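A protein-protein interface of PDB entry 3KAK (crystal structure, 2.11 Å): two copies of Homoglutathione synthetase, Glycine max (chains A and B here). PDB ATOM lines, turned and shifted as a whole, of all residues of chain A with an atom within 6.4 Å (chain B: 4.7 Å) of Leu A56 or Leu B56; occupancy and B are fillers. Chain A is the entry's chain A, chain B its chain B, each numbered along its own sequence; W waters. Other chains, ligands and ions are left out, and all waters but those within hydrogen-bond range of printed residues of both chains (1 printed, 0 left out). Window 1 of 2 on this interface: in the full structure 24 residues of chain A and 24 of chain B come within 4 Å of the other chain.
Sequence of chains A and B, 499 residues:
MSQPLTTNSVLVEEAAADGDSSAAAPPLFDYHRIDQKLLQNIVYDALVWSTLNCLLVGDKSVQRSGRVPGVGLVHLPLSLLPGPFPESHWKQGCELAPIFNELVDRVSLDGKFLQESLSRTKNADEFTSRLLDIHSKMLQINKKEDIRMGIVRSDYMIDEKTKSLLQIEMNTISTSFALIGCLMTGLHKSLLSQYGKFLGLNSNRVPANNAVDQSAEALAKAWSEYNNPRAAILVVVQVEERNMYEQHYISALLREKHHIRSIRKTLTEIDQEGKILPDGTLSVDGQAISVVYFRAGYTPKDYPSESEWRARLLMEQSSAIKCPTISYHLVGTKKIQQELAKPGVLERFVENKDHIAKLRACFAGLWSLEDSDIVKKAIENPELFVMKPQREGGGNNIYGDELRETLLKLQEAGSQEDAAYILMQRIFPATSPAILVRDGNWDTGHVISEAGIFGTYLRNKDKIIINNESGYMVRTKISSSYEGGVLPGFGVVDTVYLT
The backbone carbonyl oxygen of Gly A70 lies within hydrogen-bond range of the backbone NH of His B75, 2.9 Å away. N of Gly A70 lies close to OG1 of Thr B51 (3.2 Å). The backbone carbonyl oxygen of Thr A51 lies within hydrogen-bond range of the side-chain sulfur of Cys B54, at 3.6 Å. O of Leu B73 lies within hydrogen-bond range of N of Leu A73 (3.4 Å). The backbone carbonyl oxygen (O) of Thr B51 sits at hydrogen-bond distance from the side-chain sulfur (SG) of Cys A54 (3.3 Å).
The side-chain hydroxyl of Tyr A245 lies within hydrogen-bond range of the backbone NH of Gly A70 (2.8 Å). O of Val B74 lies within hydrogen-bond range of N of Val B57, at 2.9 Å. The backbone carbonyl oxygen of Leu A47 is in hydrogen-bond range of the side-chain hydroxyl of Thr A51 (2.9 Å).
Among the printed residues, pairs that only touch across the chains: Tyr A245 with Thr B51 (3.2 Å), Gly A70 with Val B74 (3.4 Å), Thr A51 with Tyr B245 (3.5 Å), Thr A51 with Leu B73 (3.5 Å), Leu A73 with Leu B56 (3.6 Å), Leu A56 with Leu B56 (3.6 Å), Leu A52 with Tyr B245 (3.7 Å), Leu A73 with Thr B51 (3.7 Å), Leu A52 with Cys B54 (3.8 Å) and Leu A56 with Leu B73 (3.8 Å).
Of chain B, only Leu B56 (3.6 Å) and Leu B73 (3.8 Å) come within 4 Å of Leu A56. Leu B56 touches two residues of chain A. Printed residues of chain B within 4 Å of Tyr A245: Thr B51 (3.2 Å). Printed residues of chain A within 4 Å of Leu B73: Thr A51, Leu A56 and Leu A73. Leu B55 touches none of the printed residues of chain A. The nearest printed residue of chain A that does not touch His B75 is Leu A73 (4.9 Å).
Of the 22 printed residues of chain A, 7 touch a printed residue of chain B. Of the 12 printed residues of chain B, 7 touch a printed residue of chain A. Hydrophobic or aromatic side chains of chain B within 4 Å of the printed part of chain A: Leu B56, Leu B73, Val B74, His B75 and Tyr B245. Among the printed residues, 15 pairs touch across the chains.
Thr A51 touches Cys B54, and with the chains exchanged Cys A54 touches Thr B51. Thr A51 touches Leu B73, and with the chains exchanged Leu A73 touches Thr B51. Thr A51 touches Tyr B245, and with the chains exchanged Tyr A245 touches Thr B51. Leu A56 touches Leu B73, and with the chains exchanged Leu A73 touches Leu B56. Positions printed for both chains: 50, 51, 54, 55, 56, 57, 58, 73, 74, 75, 76 and 245.
Water W1 lies within hydrogen-bond range of O of Thr A51 (2.9 Å), O of Thr B51 (3.0 Å) and N of Cys B54 (3.1 Å).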
ATOM      1  N   LEU A  47      27.244 -22.127   2.092  1.00  0.00           N
ATOM      2  CA  LEU A  47      26.571 -20.988   2.674  1.00  0.00           C
ATOM      3  C   LEU A  47      27.338 -20.416   3.896  1.00  0.00           C
ATOM      4  O   LEU A  47      27.436 -19.183   4.126  1.00  0.00           O
ATOM      5  CB  LEU A  47      25.171 -21.433   3.057  1.00  0.00           C
ATOM      6  CG  LEU A  47      24.238 -21.667   1.859  1.00  0.00           C
ATOM      7  CD1 LEU A  47      22.826 -22.112   2.291  1.00  0.00           C
ATOM      8  CD2 LEU A  47      24.144 -20.343   1.073  1.00  0.00           C
ATOM      9  N   SER A  50      30.592 -18.605   2.383  1.00  0.00           N
ATOM     10  CA  SER A  50      30.226 -17.301   1.792  1.00  0.00           C
ATOM     11  C   SER A  50      30.075 -16.265   2.917  1.00  0.00           C
ATOM     12  O   SER A  50      30.495 -15.141   2.794  1.00  0.00           O
ATOM     13  CB  SER A  50      28.863 -17.459   1.081  1.00  0.00           C
ATOM     14  OG  SER A  50      28.945 -18.332  -0.052  1.00  0.00           O
ATOM     15  N   THR A  51      29.499 -16.648   4.053  1.00  0.00           N
ATOM     16  CA  THR A  51      29.308 -15.662   5.129  1.00  0.00           C
ATOM     17  C   THR A  51      30.688 -15.378   5.674  1.00  0.00           C
ATOM     18  O   THR A  51      31.041 -14.252   5.818  1.00  0.00           O
ATOM     19  CB  THR A  51      28.318 -16.124   6.201  1.00  0.00           C
ATOM     20  OG1 THR A  51      27.122 -16.661   5.549  1.00  0.00           O
ATOM     21  CG2 THR A  51      27.896 -14.982   7.078  1.00  0.00           C
ATOM     22  N   LEU A  52      31.489 -16.395   5.935  1.00  0.00           N
ATOM     23  CA  LEU A  52      32.752 -16.124   6.633  1.00  0.00           C
ATOM     24  C   LEU A  52      33.702 -15.308   5.834  1.00  0.00           C
ATOM     25  O   LEU A  52      34.639 -14.676   6.383  1.00  0.00           O
ATOM     26  CB  LEU A  52      33.445 -17.401   7.102  1.00  0.00           C
ATOM     27  CG  LEU A  52      32.733 -18.098   8.294  1.00  0.00           C
ATOM     28  CD1 LEU A  52      33.340 -19.478   8.345  1.00  0.00           C
ATOM     29  CD2 LEU A  52      32.912 -17.411   9.690  1.00  0.00           C
ATOM     30  N   ASN A  53      33.543 -15.371   4.529  1.00  0.00           N
ATOM     31  CA  ASN A  53      34.509 -14.807   3.637  1.00  0.00           C
ATOM     32  C   ASN A  53      33.939 -13.611   2.848  1.00  0.00           C
ATOM     33  O   ASN A  53      34.557 -13.145   1.871  1.00  0.00           O
ATOM     34  CB  ASN A  53      35.047 -15.862   2.699  1.00  0.00           C
ATOM     35  CG  ASN A  53      35.990 -16.830   3.384  1.00  0.00           C
ATOM     36  OD1 ASN A  53      37.189 -16.640   3.365  1.00  0.00           O
ATOM     37  ND2 ASN A  53      35.442 -17.863   3.997  1.00  0.00           N
ATOM     38  N   CYS A  54      32.732 -13.132   3.208  1.00  0.00           N
ATOM     39  CA  CYS A  54      32.215 -11.959   2.532  1.00  0.00           C
ATOM     40  C   CYS A  54      31.967 -12.109   1.046  1.00  0.00           C
ATOM     41  O   CYS A  54      32.205 -11.173   0.238  1.00  0.00           O
ATOM     42  CB  CYS A  54      32.997 -10.633   2.773  1.00  0.00           C
ATOM     43  SG  CYS A  54      31.790  -9.101   2.704  1.00  0.00           S
ATOM     44  N   LEU A  55      31.409 -13.232   0.709  1.00  0.00           N
ATOM     45  CA  LEU A  55      30.752 -13.427  -0.544  1.00  0.00           C
ATOM     46  C   LEU A  55      29.347 -12.933  -0.300  1.00  0.00           C
ATOM     47  O   LEU A  55      28.416 -13.722  -0.338  1.00  0.00           O
ATOM     48  CB  LEU A  55      30.709 -14.928  -0.890  1.00  0.00           C
ATOM     49  CG  LEU A  55      30.381 -14.974  -2.361  1.00  0.00           C
ATOM     50  CD1 LEU A  55      31.177 -13.946  -3.065  1.00  0.00           C
ATOM     51  CD2 LEU A  55      30.632 -16.400  -2.972  1.00  0.00           C
ATOM     52  N   LEU A  56      29.232 -11.631  -0.094  1.00  0.00           N
ATOM     53  CA  LEU A  56      27.957 -11.047   0.353  1.00  0.00           C
ATOM     54  C   LEU A  56      27.567  -9.763  -0.360  1.00  0.00           C
ATOM     55  O   LEU A  56      28.431  -8.928  -0.816  1.00  0.00           O
ATOM     56  CB  LEU A  56      27.922 -10.797   1.863  1.00  0.00           C
ATOM     57  CG  LEU A  56      28.134 -11.954   2.815  1.00  0.00           C
ATOM     58  CD1 LEU A  56      28.416 -11.402   4.277  1.00  0.00           C
ATOM     59  CD2 LEU A  56      26.967 -12.988   2.781  1.00  0.00           C
ATOM     60  N   VAL A  57      26.248  -9.624  -0.504  1.00  0.00           N
ATOM     61  CA  VAL A  57      25.719  -8.424  -1.120  1.00  0.00           C
ATOM     62  C   VAL A  57      24.463  -8.019  -0.321  1.00  0.00           C
ATOM     63  O   VAL A  57      23.923  -8.823   0.421  1.00  0.00           O
ATOM     64  CB  VAL A  57      25.371  -8.662  -2.566  1.00  0.00           C
ATOM     65  CG1 VAL A  57      26.607  -8.663  -3.448  1.00  0.00           C
ATOM     66  CG2 VAL A  57      24.617  -9.976  -2.655  1.00  0.00           C
ATOM     67  N   GLY A  58      24.067  -6.746  -0.445  1.00  0.00           N
ATOM     68  CA  GLY A  58      22.779  -6.288  -0.011  1.00  0.00           C
ATOM     69  C   GLY A  58      21.654  -7.114  -0.640  1.00  0.00           C
ATOM     70  O   GLY A  58      21.610  -7.412  -1.845  1.00  0.00           O
ATOM     71  N   GLY A  70      26.354  -3.281   6.328  1.00  0.00           N
ATOM     72  CA  GLY A  70      26.248  -3.965   7.639  1.00  0.00           C
ATOM     73  C   GLY A  70      24.841  -4.456   7.956  1.00  0.00           C
ATOM     74  O   GLY A  70      24.625  -5.092   9.025  1.00  0.00           O
ATOM     75  N   LEU A  73      21.951  -8.122   4.567  1.00  0.00           N
ATOM     76  CA  LEU A  73      23.058  -8.820   3.870  1.00  0.00           C
ATOM     77  C   LEU A  73      22.653 -10.210   3.451  1.00  0.00           C
ATOM     78  O   LEU A  73      21.846 -10.900   4.156  1.00  0.00           O
ATOM     79  CB  LEU A  73      24.265  -8.951   4.857  1.00  0.00           C
ATOM     80  CG  LEU A  73      25.017  -7.615   5.064  1.00  0.00           C
ATOM     81  CD1 LEU A  73      25.810  -7.536   6.453  1.00  0.00           C
ATOM     82  CD2 LEU A  73      25.931  -7.306   3.844  1.00  0.00           C
ATOM     83  N   VAL A  74      23.206 -10.688   2.357  1.00  0.00           N
ATOM     84  CA  VAL A  74      22.816 -12.012   1.851  1.00  0.00           C
ATOM     85  C   VAL A  74      23.958 -12.589   0.973  1.00  0.00           C
ATOM     86  O   VAL A  74      24.748 -11.805   0.437  1.00  0.00           O
ATOM     87  CB  VAL A  74      21.367 -12.019   1.235  1.00  0.00           C
ATOM     88  CG1 VAL A  74      21.291 -11.310  -0.139  1.00  0.00           C
ATOM     89  CG2 VAL A  74      20.786 -13.443   1.149  1.00  0.00           C
ATOM     90  N   HIS A  75      24.088 -13.917   0.880  1.00  0.00           N
ATOM     91  CA  HIS A  75      25.167 -14.500   0.087  1.00  0.00           C
ATOM     92  C   HIS A  75      24.880 -14.131  -1.334  1.00  0.00           C
ATOM     93  O   HIS A  75      23.704 -13.992  -1.654  1.00  0.00           O
ATOM     94  CB  HIS A  75      25.252 -16.052   0.225  1.00  0.00           C
ATOM     95  CG  HIS A  75      24.015 -16.783  -0.225  1.00  0.00           C
ATOM     96  ND1 HIS A  75      23.900 -17.370  -1.472  1.00  0.00           N
ATOM     97  CD2 HIS A  75      22.846 -17.048   0.430  1.00  0.00           C
ATOM     98  CE1 HIS A  75      22.704 -17.945  -1.574  1.00  0.00           C
ATOM     99  NE2 HIS A  75      22.033 -17.738  -0.441  1.00  0.00           N
ATOM    100  N   LEU A  76      25.910 -13.934  -2.164  1.00  0.00           N
ATOM    101  CA  LEU A  76      25.750 -13.859  -3.627  1.00  0.00           C
ATOM    102  C   LEU A  76      25.041 -15.095  -4.154  1.00  0.00           C
ATOM    103  O   LEU A  76      25.398 -16.222  -3.719  1.00  0.00           O
ATOM    104  CB  LEU A  76      27.112 -13.852  -4.364  1.00  0.00           C
ATOM    105  CG  LEU A  76      27.823 -12.579  -4.776  1.00  0.00           C
ATOM    106  CD1 LEU A  76      26.823 -11.720  -5.571  1.00  0.00           C
ATOM    107  CD2 LEU A  76      28.271 -11.967  -3.457  1.00  0.00           C
ATOM    108  N   ILE A 180      34.356 -10.945  -6.103  1.00  0.00           N
ATOM    109  CA  ILE A 180      33.436 -12.018  -6.199  1.00  0.00           C
ATOM    110  C   ILE A 180      34.013 -13.217  -6.912  1.00  0.00           C
ATOM    111  O   ILE A 180      33.815 -14.352  -6.491  1.00  0.00           O
ATOM    112  CB  ILE A 180      32.170 -11.587  -6.959  1.00  0.00           C
ATOM    113  CG1 ILE A 180      31.318 -10.538  -6.198  1.00  0.00           C
ATOM    114  CG2 ILE A 180      31.324 -12.812  -7.210  1.00  0.00           C
ATOM    115  CD1 ILE A 180      31.892  -9.957  -4.919  1.00  0.00           C
ATOM    116  N   LEU A 183      36.533 -14.884  -4.595  1.00  0.00           N
ATOM    117  CA  LEU A 183      35.962 -15.637  -3.458  1.00  0.00           C
ATOM    118  C   LEU A 183      35.335 -16.914  -3.967  1.00  0.00           C
ATOM    119  O   LEU A 183      35.269 -17.907  -3.263  1.00  0.00           O
ATOM    120  CB  LEU A 183      34.937 -14.820  -2.693  1.00  0.00           C
ATOM    121  CG  LEU A 183      35.480 -13.558  -2.010  1.00  0.00           C
ATOM    122  CD1 LEU A 183      34.299 -12.566  -1.648  1.00  0.00           C
ATOM    123  CD2 LEU A 183      36.307 -13.893  -0.793  1.00  0.00           C
ATOM    124  N   ARG A 242      24.431  -2.268  -3.815  1.00  0.00           N
ATOM    125  CA  ARG A 242      24.320  -3.506  -3.072  1.00  0.00           C
ATOM    126  C   ARG A 242      25.609  -4.296  -3.134  1.00  0.00           C
ATOM    127  O   ARG A 242      25.920  -5.025  -2.175  1.00  0.00           O
ATOM    128  CB  ARG A 242      23.162  -4.347  -3.569  1.00  0.00           C
ATOM    129  CG  ARG A 242      21.841  -3.615  -3.471  1.00  0.00           C
ATOM    130  CD  ARG A 242      20.720  -4.571  -3.623  1.00  0.00           C
ATOM    131  NE  ARG A 242      20.549  -5.049  -4.993  1.00  0.00           N
ATOM    132  CZ  ARG A 242      21.013  -6.215  -5.454  1.00  0.00           C
ATOM    133  NH1 ARG A 242      20.746  -6.541  -6.698  1.00  0.00           N
ATOM    134  NH2 ARG A 242      21.747  -7.056  -4.694  1.00  0.00           N
ATOM    135  N   ASN A 243      26.357  -4.124  -4.234  1.00  0.00           N
ATOM    136  CA  ASN A 243      27.695  -4.722  -4.330  1.00  0.00           C
ATOM    137  C   ASN A 243      28.792  -3.799  -3.728  1.00  0.00           C
ATOM    138  O   ASN A 243      29.926  -3.870  -4.124  1.00  0.00           O
ATOM    139  CB  ASN A 243      27.974  -5.091  -5.792  1.00  0.00           C
ATOM    140  CG  ASN A 243      29.225  -5.960  -6.002  1.00  0.00           C
ATOM    141  OD1 ASN A 243      29.607  -6.912  -5.216  1.00  0.00           O
ATOM    142  ND2 ASN A 243      29.875  -5.657  -7.106  1.00  0.00           N
ATOM    143  N   MET A 244      28.467  -2.952  -2.752  1.00  0.00           N
ATOM    144  CA  MET A 244      29.479  -2.037  -2.250  1.00  0.00           C
ATOM    145  C   MET A 244      30.671  -2.792  -1.619  1.00  0.00           C
ATOM    146  O   MET A 244      31.791  -2.249  -1.507  1.00  0.00           O
ATOM    147  CB  MET A 244      28.890  -1.058  -1.240  1.00  0.00           C
ATOM    148  CG  MET A 244      28.288  -1.811  -0.024  1.00  0.00           C
ATOM    149  SD  MET A 244      27.799  -0.749   1.309  1.00  0.00           S
ATOM    150  CE  MET A 244      26.372   0.093   0.665  1.00  0.00           C
ATOM    151  N   TYR A 245      30.475  -4.027  -1.203  1.00  0.00           N
ATOM    152  CA  TYR A 245      31.560  -4.635  -0.404  1.00  0.00           C
ATOM    153  C   TYR A 245      32.781  -5.013  -1.291  1.00  0.00           C
ATOM    154  O   TYR A 245      33.919  -4.926  -0.864  1.00  0.00           O
ATOM    155  CB  TYR A 245      30.959  -5.759   0.476  1.00  0.00           C
ATOM    156  CG  TYR A 245      29.834  -5.214   1.353  1.00  0.00           C
ATOM    157  CD1 TYR A 245      28.530  -5.380   1.005  1.00  0.00           C
ATOM    158  CD2 TYR A 245      30.100  -4.499   2.516  1.00  0.00           C
ATOM    159  CE1 TYR A 245      27.475  -4.837   1.748  1.00  0.00           C
ATOM    160  CE2 TYR A 245      29.016  -3.972   3.293  1.00  0.00           C
ATOM    161  CZ  TYR A 245      27.708  -4.158   2.862  1.00  0.00           C
ATOM    162  OH  TYR A 245      26.598  -3.716   3.575  1.00  0.00           O
ATOM    163  N   GLU A 246      32.561  -5.307  -2.581  1.00  0.00           N
ATOM    164  CA  GLU A 246      33.686  -5.493  -3.459  1.00  0.00           C
ATOM    165  C   GLU A 246      34.601  -4.267  -3.436  1.00  0.00           C
ATOM    166  O   GLU A 246      35.842  -4.384  -3.307  1.00  0.00           O
ATOM    167  CB  GLU A 246      33.181  -5.769  -4.858  1.00  0.00           C
ATOM    168  CG  GLU A 246      34.298  -6.046  -5.897  1.00  0.00           C
ATOM    169  CD  GLU A 246      33.739  -6.765  -7.025  1.00  0.00           C
ATOM    170  OE1 GLU A 246      32.887  -6.210  -7.771  1.00  0.00           O
ATOM    171  OE2 GLU A 246      34.032  -7.929  -7.071  1.00  0.00           O
ATOM    172  N   SER B  50      32.982  -4.312   9.709  1.00  0.00           N
ATOM    173  CA  SER B  50      32.155  -5.394  10.243  1.00  0.00           C
ATOM    174  C   SER B  50      31.708  -6.390   9.144  1.00  0.00           C
ATOM    175  O   SER B  50      31.693  -7.624   9.321  1.00  0.00           O
ATOM    176  CB  SER B  50      30.954  -4.812  11.001  1.00  0.00           C
ATOM    177  OG  SER B  50      31.465  -3.923  12.020  1.00  0.00           O
ATOM    178  N   THR B  51      31.360  -5.837   8.000  1.00  0.00           N
ATOM    179  CA  THR B  51      30.836  -6.685   6.939  1.00  0.00           C
ATOM    180  C   THR B  51      31.971  -7.453   6.246  1.00  0.00           C
ATOM    181  O   THR B  51      31.827  -8.653   5.928  1.00  0.00           O
ATOM    182  CB  THR B  51      29.970  -5.828   5.944  1.00  0.00           C
ATOM    183  OG1 THR B  51      28.911  -5.151   6.699  1.00  0.00           O
ATOM    184  CG2 THR B  51      29.399  -6.714   4.989  1.00  0.00           C
ATOM    185  N   CYS B  54      33.392 -10.314   8.837  1.00  0.00           N
ATOM    186  CA  CYS B  54      32.420 -11.252   9.426  1.00  0.00           C
ATOM    187  C   CYS B  54      32.189 -10.980  10.911  1.00  0.00           C
ATOM    188  O   CYS B  54      32.086 -11.897  11.707  1.00  0.00           O
ATOM    189  CB  CYS B  54      32.777 -12.706   9.306  1.00  0.00           C
ATOM    190  SG  CYS B  54      31.359 -13.862   9.370  1.00  0.00           S
ATOM    191  N   LEU B  55      32.045  -9.732  11.245  1.00  0.00           N
ATOM    192  CA  LEU B  55      31.529  -9.406  12.606  1.00  0.00           C
ATOM    193  C   LEU B  55      30.013  -9.354  12.451  1.00  0.00           C
ATOM    194  O   LEU B  55      29.428  -8.278  12.484  1.00  0.00           O
ATOM    195  CB  LEU B  55      32.074  -8.051  12.984  1.00  0.00           C
ATOM    196  CG  LEU B  55      31.706  -7.453  14.357  1.00  0.00           C
ATOM    197  CD1 LEU B  55      32.145  -8.421  15.393  1.00  0.00           C
ATOM    198  CD2 LEU B  55      32.436  -6.212  14.437  1.00  0.00           C
ATOM    199  N   LEU B  56      29.423 -10.504  12.151  1.00  0.00           N
ATOM    200  CA  LEU B  56      28.009 -10.605  11.769  1.00  0.00           C
ATOM    201  C   LEU B  56      27.312 -11.689  12.559  1.00  0.00           C
ATOM    202  O   LEU B  56      27.996 -12.653  13.013  1.00  0.00           O
ATOM    203  CB  LEU B  56      27.855 -10.881  10.283  1.00  0.00           C
ATOM    204  CG  LEU B  56      28.602 -10.076   9.204  1.00  0.00           C
ATOM    205  CD1 LEU B  56      28.484 -10.759   7.865  1.00  0.00           C
ATOM    206  CD2 LEU B  56      28.025  -8.689   9.047  1.00  0.00           C
ATOM    207  N   VAL B  57      26.003 -11.476  12.851  1.00  0.00           N
ATOM    208  CA  VAL B  57      25.129 -12.506  13.346  1.00  0.00           C
ATOM    209  C   VAL B  57      23.847 -12.565  12.537  1.00  0.00           C
ATOM    210  O   VAL B  57      23.543 -11.619  11.864  1.00  0.00           O
ATOM    211  CB  VAL B  57      24.679 -12.155  14.766  1.00  0.00           C
ATOM    212  CG1 VAL B  57      25.770 -12.616  15.763  1.00  0.00           C
ATOM    213  CG2 VAL B  57      24.391 -10.610  14.866  1.00  0.00           C
ATOM    214  N   GLY B  58      23.099 -13.674  12.605  1.00  0.00           N
ATOM    215  CA  GLY B  58      21.667 -13.698  12.261  1.00  0.00           C
ATOM    216  C   GLY B  58      20.848 -12.546  12.827  1.00  0.00           C
ATOM    217  O   GLY B  58      20.921 -12.200  14.005  1.00  0.00           O
ATOM    218  N   LEU B  73      21.684 -11.558   7.529  1.00  0.00           N
ATOM    219  CA  LEU B  73      22.832 -11.056   8.319  1.00  0.00           C
ATOM    220  C   LEU B  73      22.783  -9.598   8.641  1.00  0.00           C
ATOM    221  O   LEU B  73      22.281  -8.706   7.859  1.00  0.00           O
ATOM    222  CB  LEU B  73      24.174 -11.382   7.625  1.00  0.00           C
ATOM    223  CG  LEU B  73      24.168 -12.885   7.304  1.00  0.00           C
ATOM    224  CD1 LEU B  73      24.683 -13.163   5.856  1.00  0.00           C
ATOM    225  CD2 LEU B  73      24.851 -13.787   8.341  1.00  0.00           C
ATOM    226  N   VAL B  74      23.354  -9.332   9.811  1.00  0.00           N
ATOM    227  CA  VAL B  74      23.431  -8.023  10.335  1.00  0.00           C
ATOM    228  C   VAL B  74      24.722  -7.977  11.145  1.00  0.00           C
ATOM    229  O   VAL B  74      25.123  -8.998  11.650  1.00  0.00           O
ATOM    230  CB  VAL B  74      22.197  -7.686  11.221  1.00  0.00           C
ATOM    231  CG1 VAL B  74      22.280  -8.374  12.598  1.00  0.00           C
ATOM    232  CG2 VAL B  74      22.160  -6.153  11.438  1.00  0.00           C
ATOM    233  N   HIS B  75      25.338  -6.799  11.246  1.00  0.00           N
ATOM    234  CA  HIS B  75      26.509  -6.604  12.065  1.00  0.00           C
ATOM    235  C   HIS B  75      26.142  -6.818  13.517  1.00  0.00           C
ATOM    236  O   HIS B  75      25.030  -6.591  13.888  1.00  0.00           O
ATOM    237  CB  HIS B  75      27.084  -5.188  11.860  1.00  0.00           C
ATOM    238  CG  HIS B  75      26.238  -4.071  12.457  1.00  0.00           C
ATOM    239  ND1 HIS B  75      26.415  -3.601  13.749  1.00  0.00           N
ATOM    240  CD2 HIS B  75      25.200  -3.357  11.943  1.00  0.00           C
ATOM    241  CE1 HIS B  75      25.522  -2.666  14.006  1.00  0.00           C
ATOM    242  NE2 HIS B  75      24.793  -2.480  12.924  1.00  0.00           N
ATOM    243  N   LEU B  76      27.093  -7.247  14.329  1.00  0.00           N
ATOM    244  CA  LEU B  76      26.946  -7.177  15.800  1.00  0.00           C
ATOM    245  C   LEU B  76      26.645  -5.766  16.277  1.00  0.00           C
ATOM    246  O   LEU B  76      27.211  -4.791  15.704  1.00  0.00           O
ATOM    247  CB  LEU B  76      28.216  -7.682  16.527  1.00  0.00           C
ATOM    248  CG  LEU B  76      28.260  -9.188  16.812  1.00  0.00           C
ATOM    249  CD1 LEU B  76      27.048  -9.609  17.670  1.00  0.00           C
ATOM    250  CD2 LEU B  76      28.388  -9.961  15.465  1.00  0.00           C
ATOM    251  N   TYR B 245      28.370 -18.140  13.392  1.00  0.00           N
ATOM    252  CA  TYR B 245      29.635 -17.785  12.653  1.00  0.00           C
ATOM    253  C   TYR B 245      30.873 -17.871  13.527  1.00  0.00           C
ATOM    254  O   TYR B 245      32.011 -18.312  13.129  1.00  0.00           O
ATOM    255  CB  TYR B 245      29.517 -16.413  11.939  1.00  0.00           C
ATOM    256  CG  TYR B 245      28.382 -16.543  11.012  1.00  0.00           C
ATOM    257  CD1 TYR B 245      27.169 -15.952  11.360  1.00  0.00           C
ATOM    258  CD2 TYR B 245      28.408 -17.460   9.932  1.00  0.00           C
ATOM    259  CE1 TYR B 245      26.077 -16.138  10.690  1.00  0.00           C
ATOM    260  CE2 TYR B 245      27.221 -17.655   9.189  1.00  0.00           C
ATOM    261  CZ  TYR B 245      26.059 -16.940   9.609  1.00  0.00           C
ATOM    262  OH  TYR B 245      24.796 -17.028   9.038  1.00  0.00           O
HETATM  263  O   HOH W   1      32.140 -11.596   6.298  1.00  0.00           O
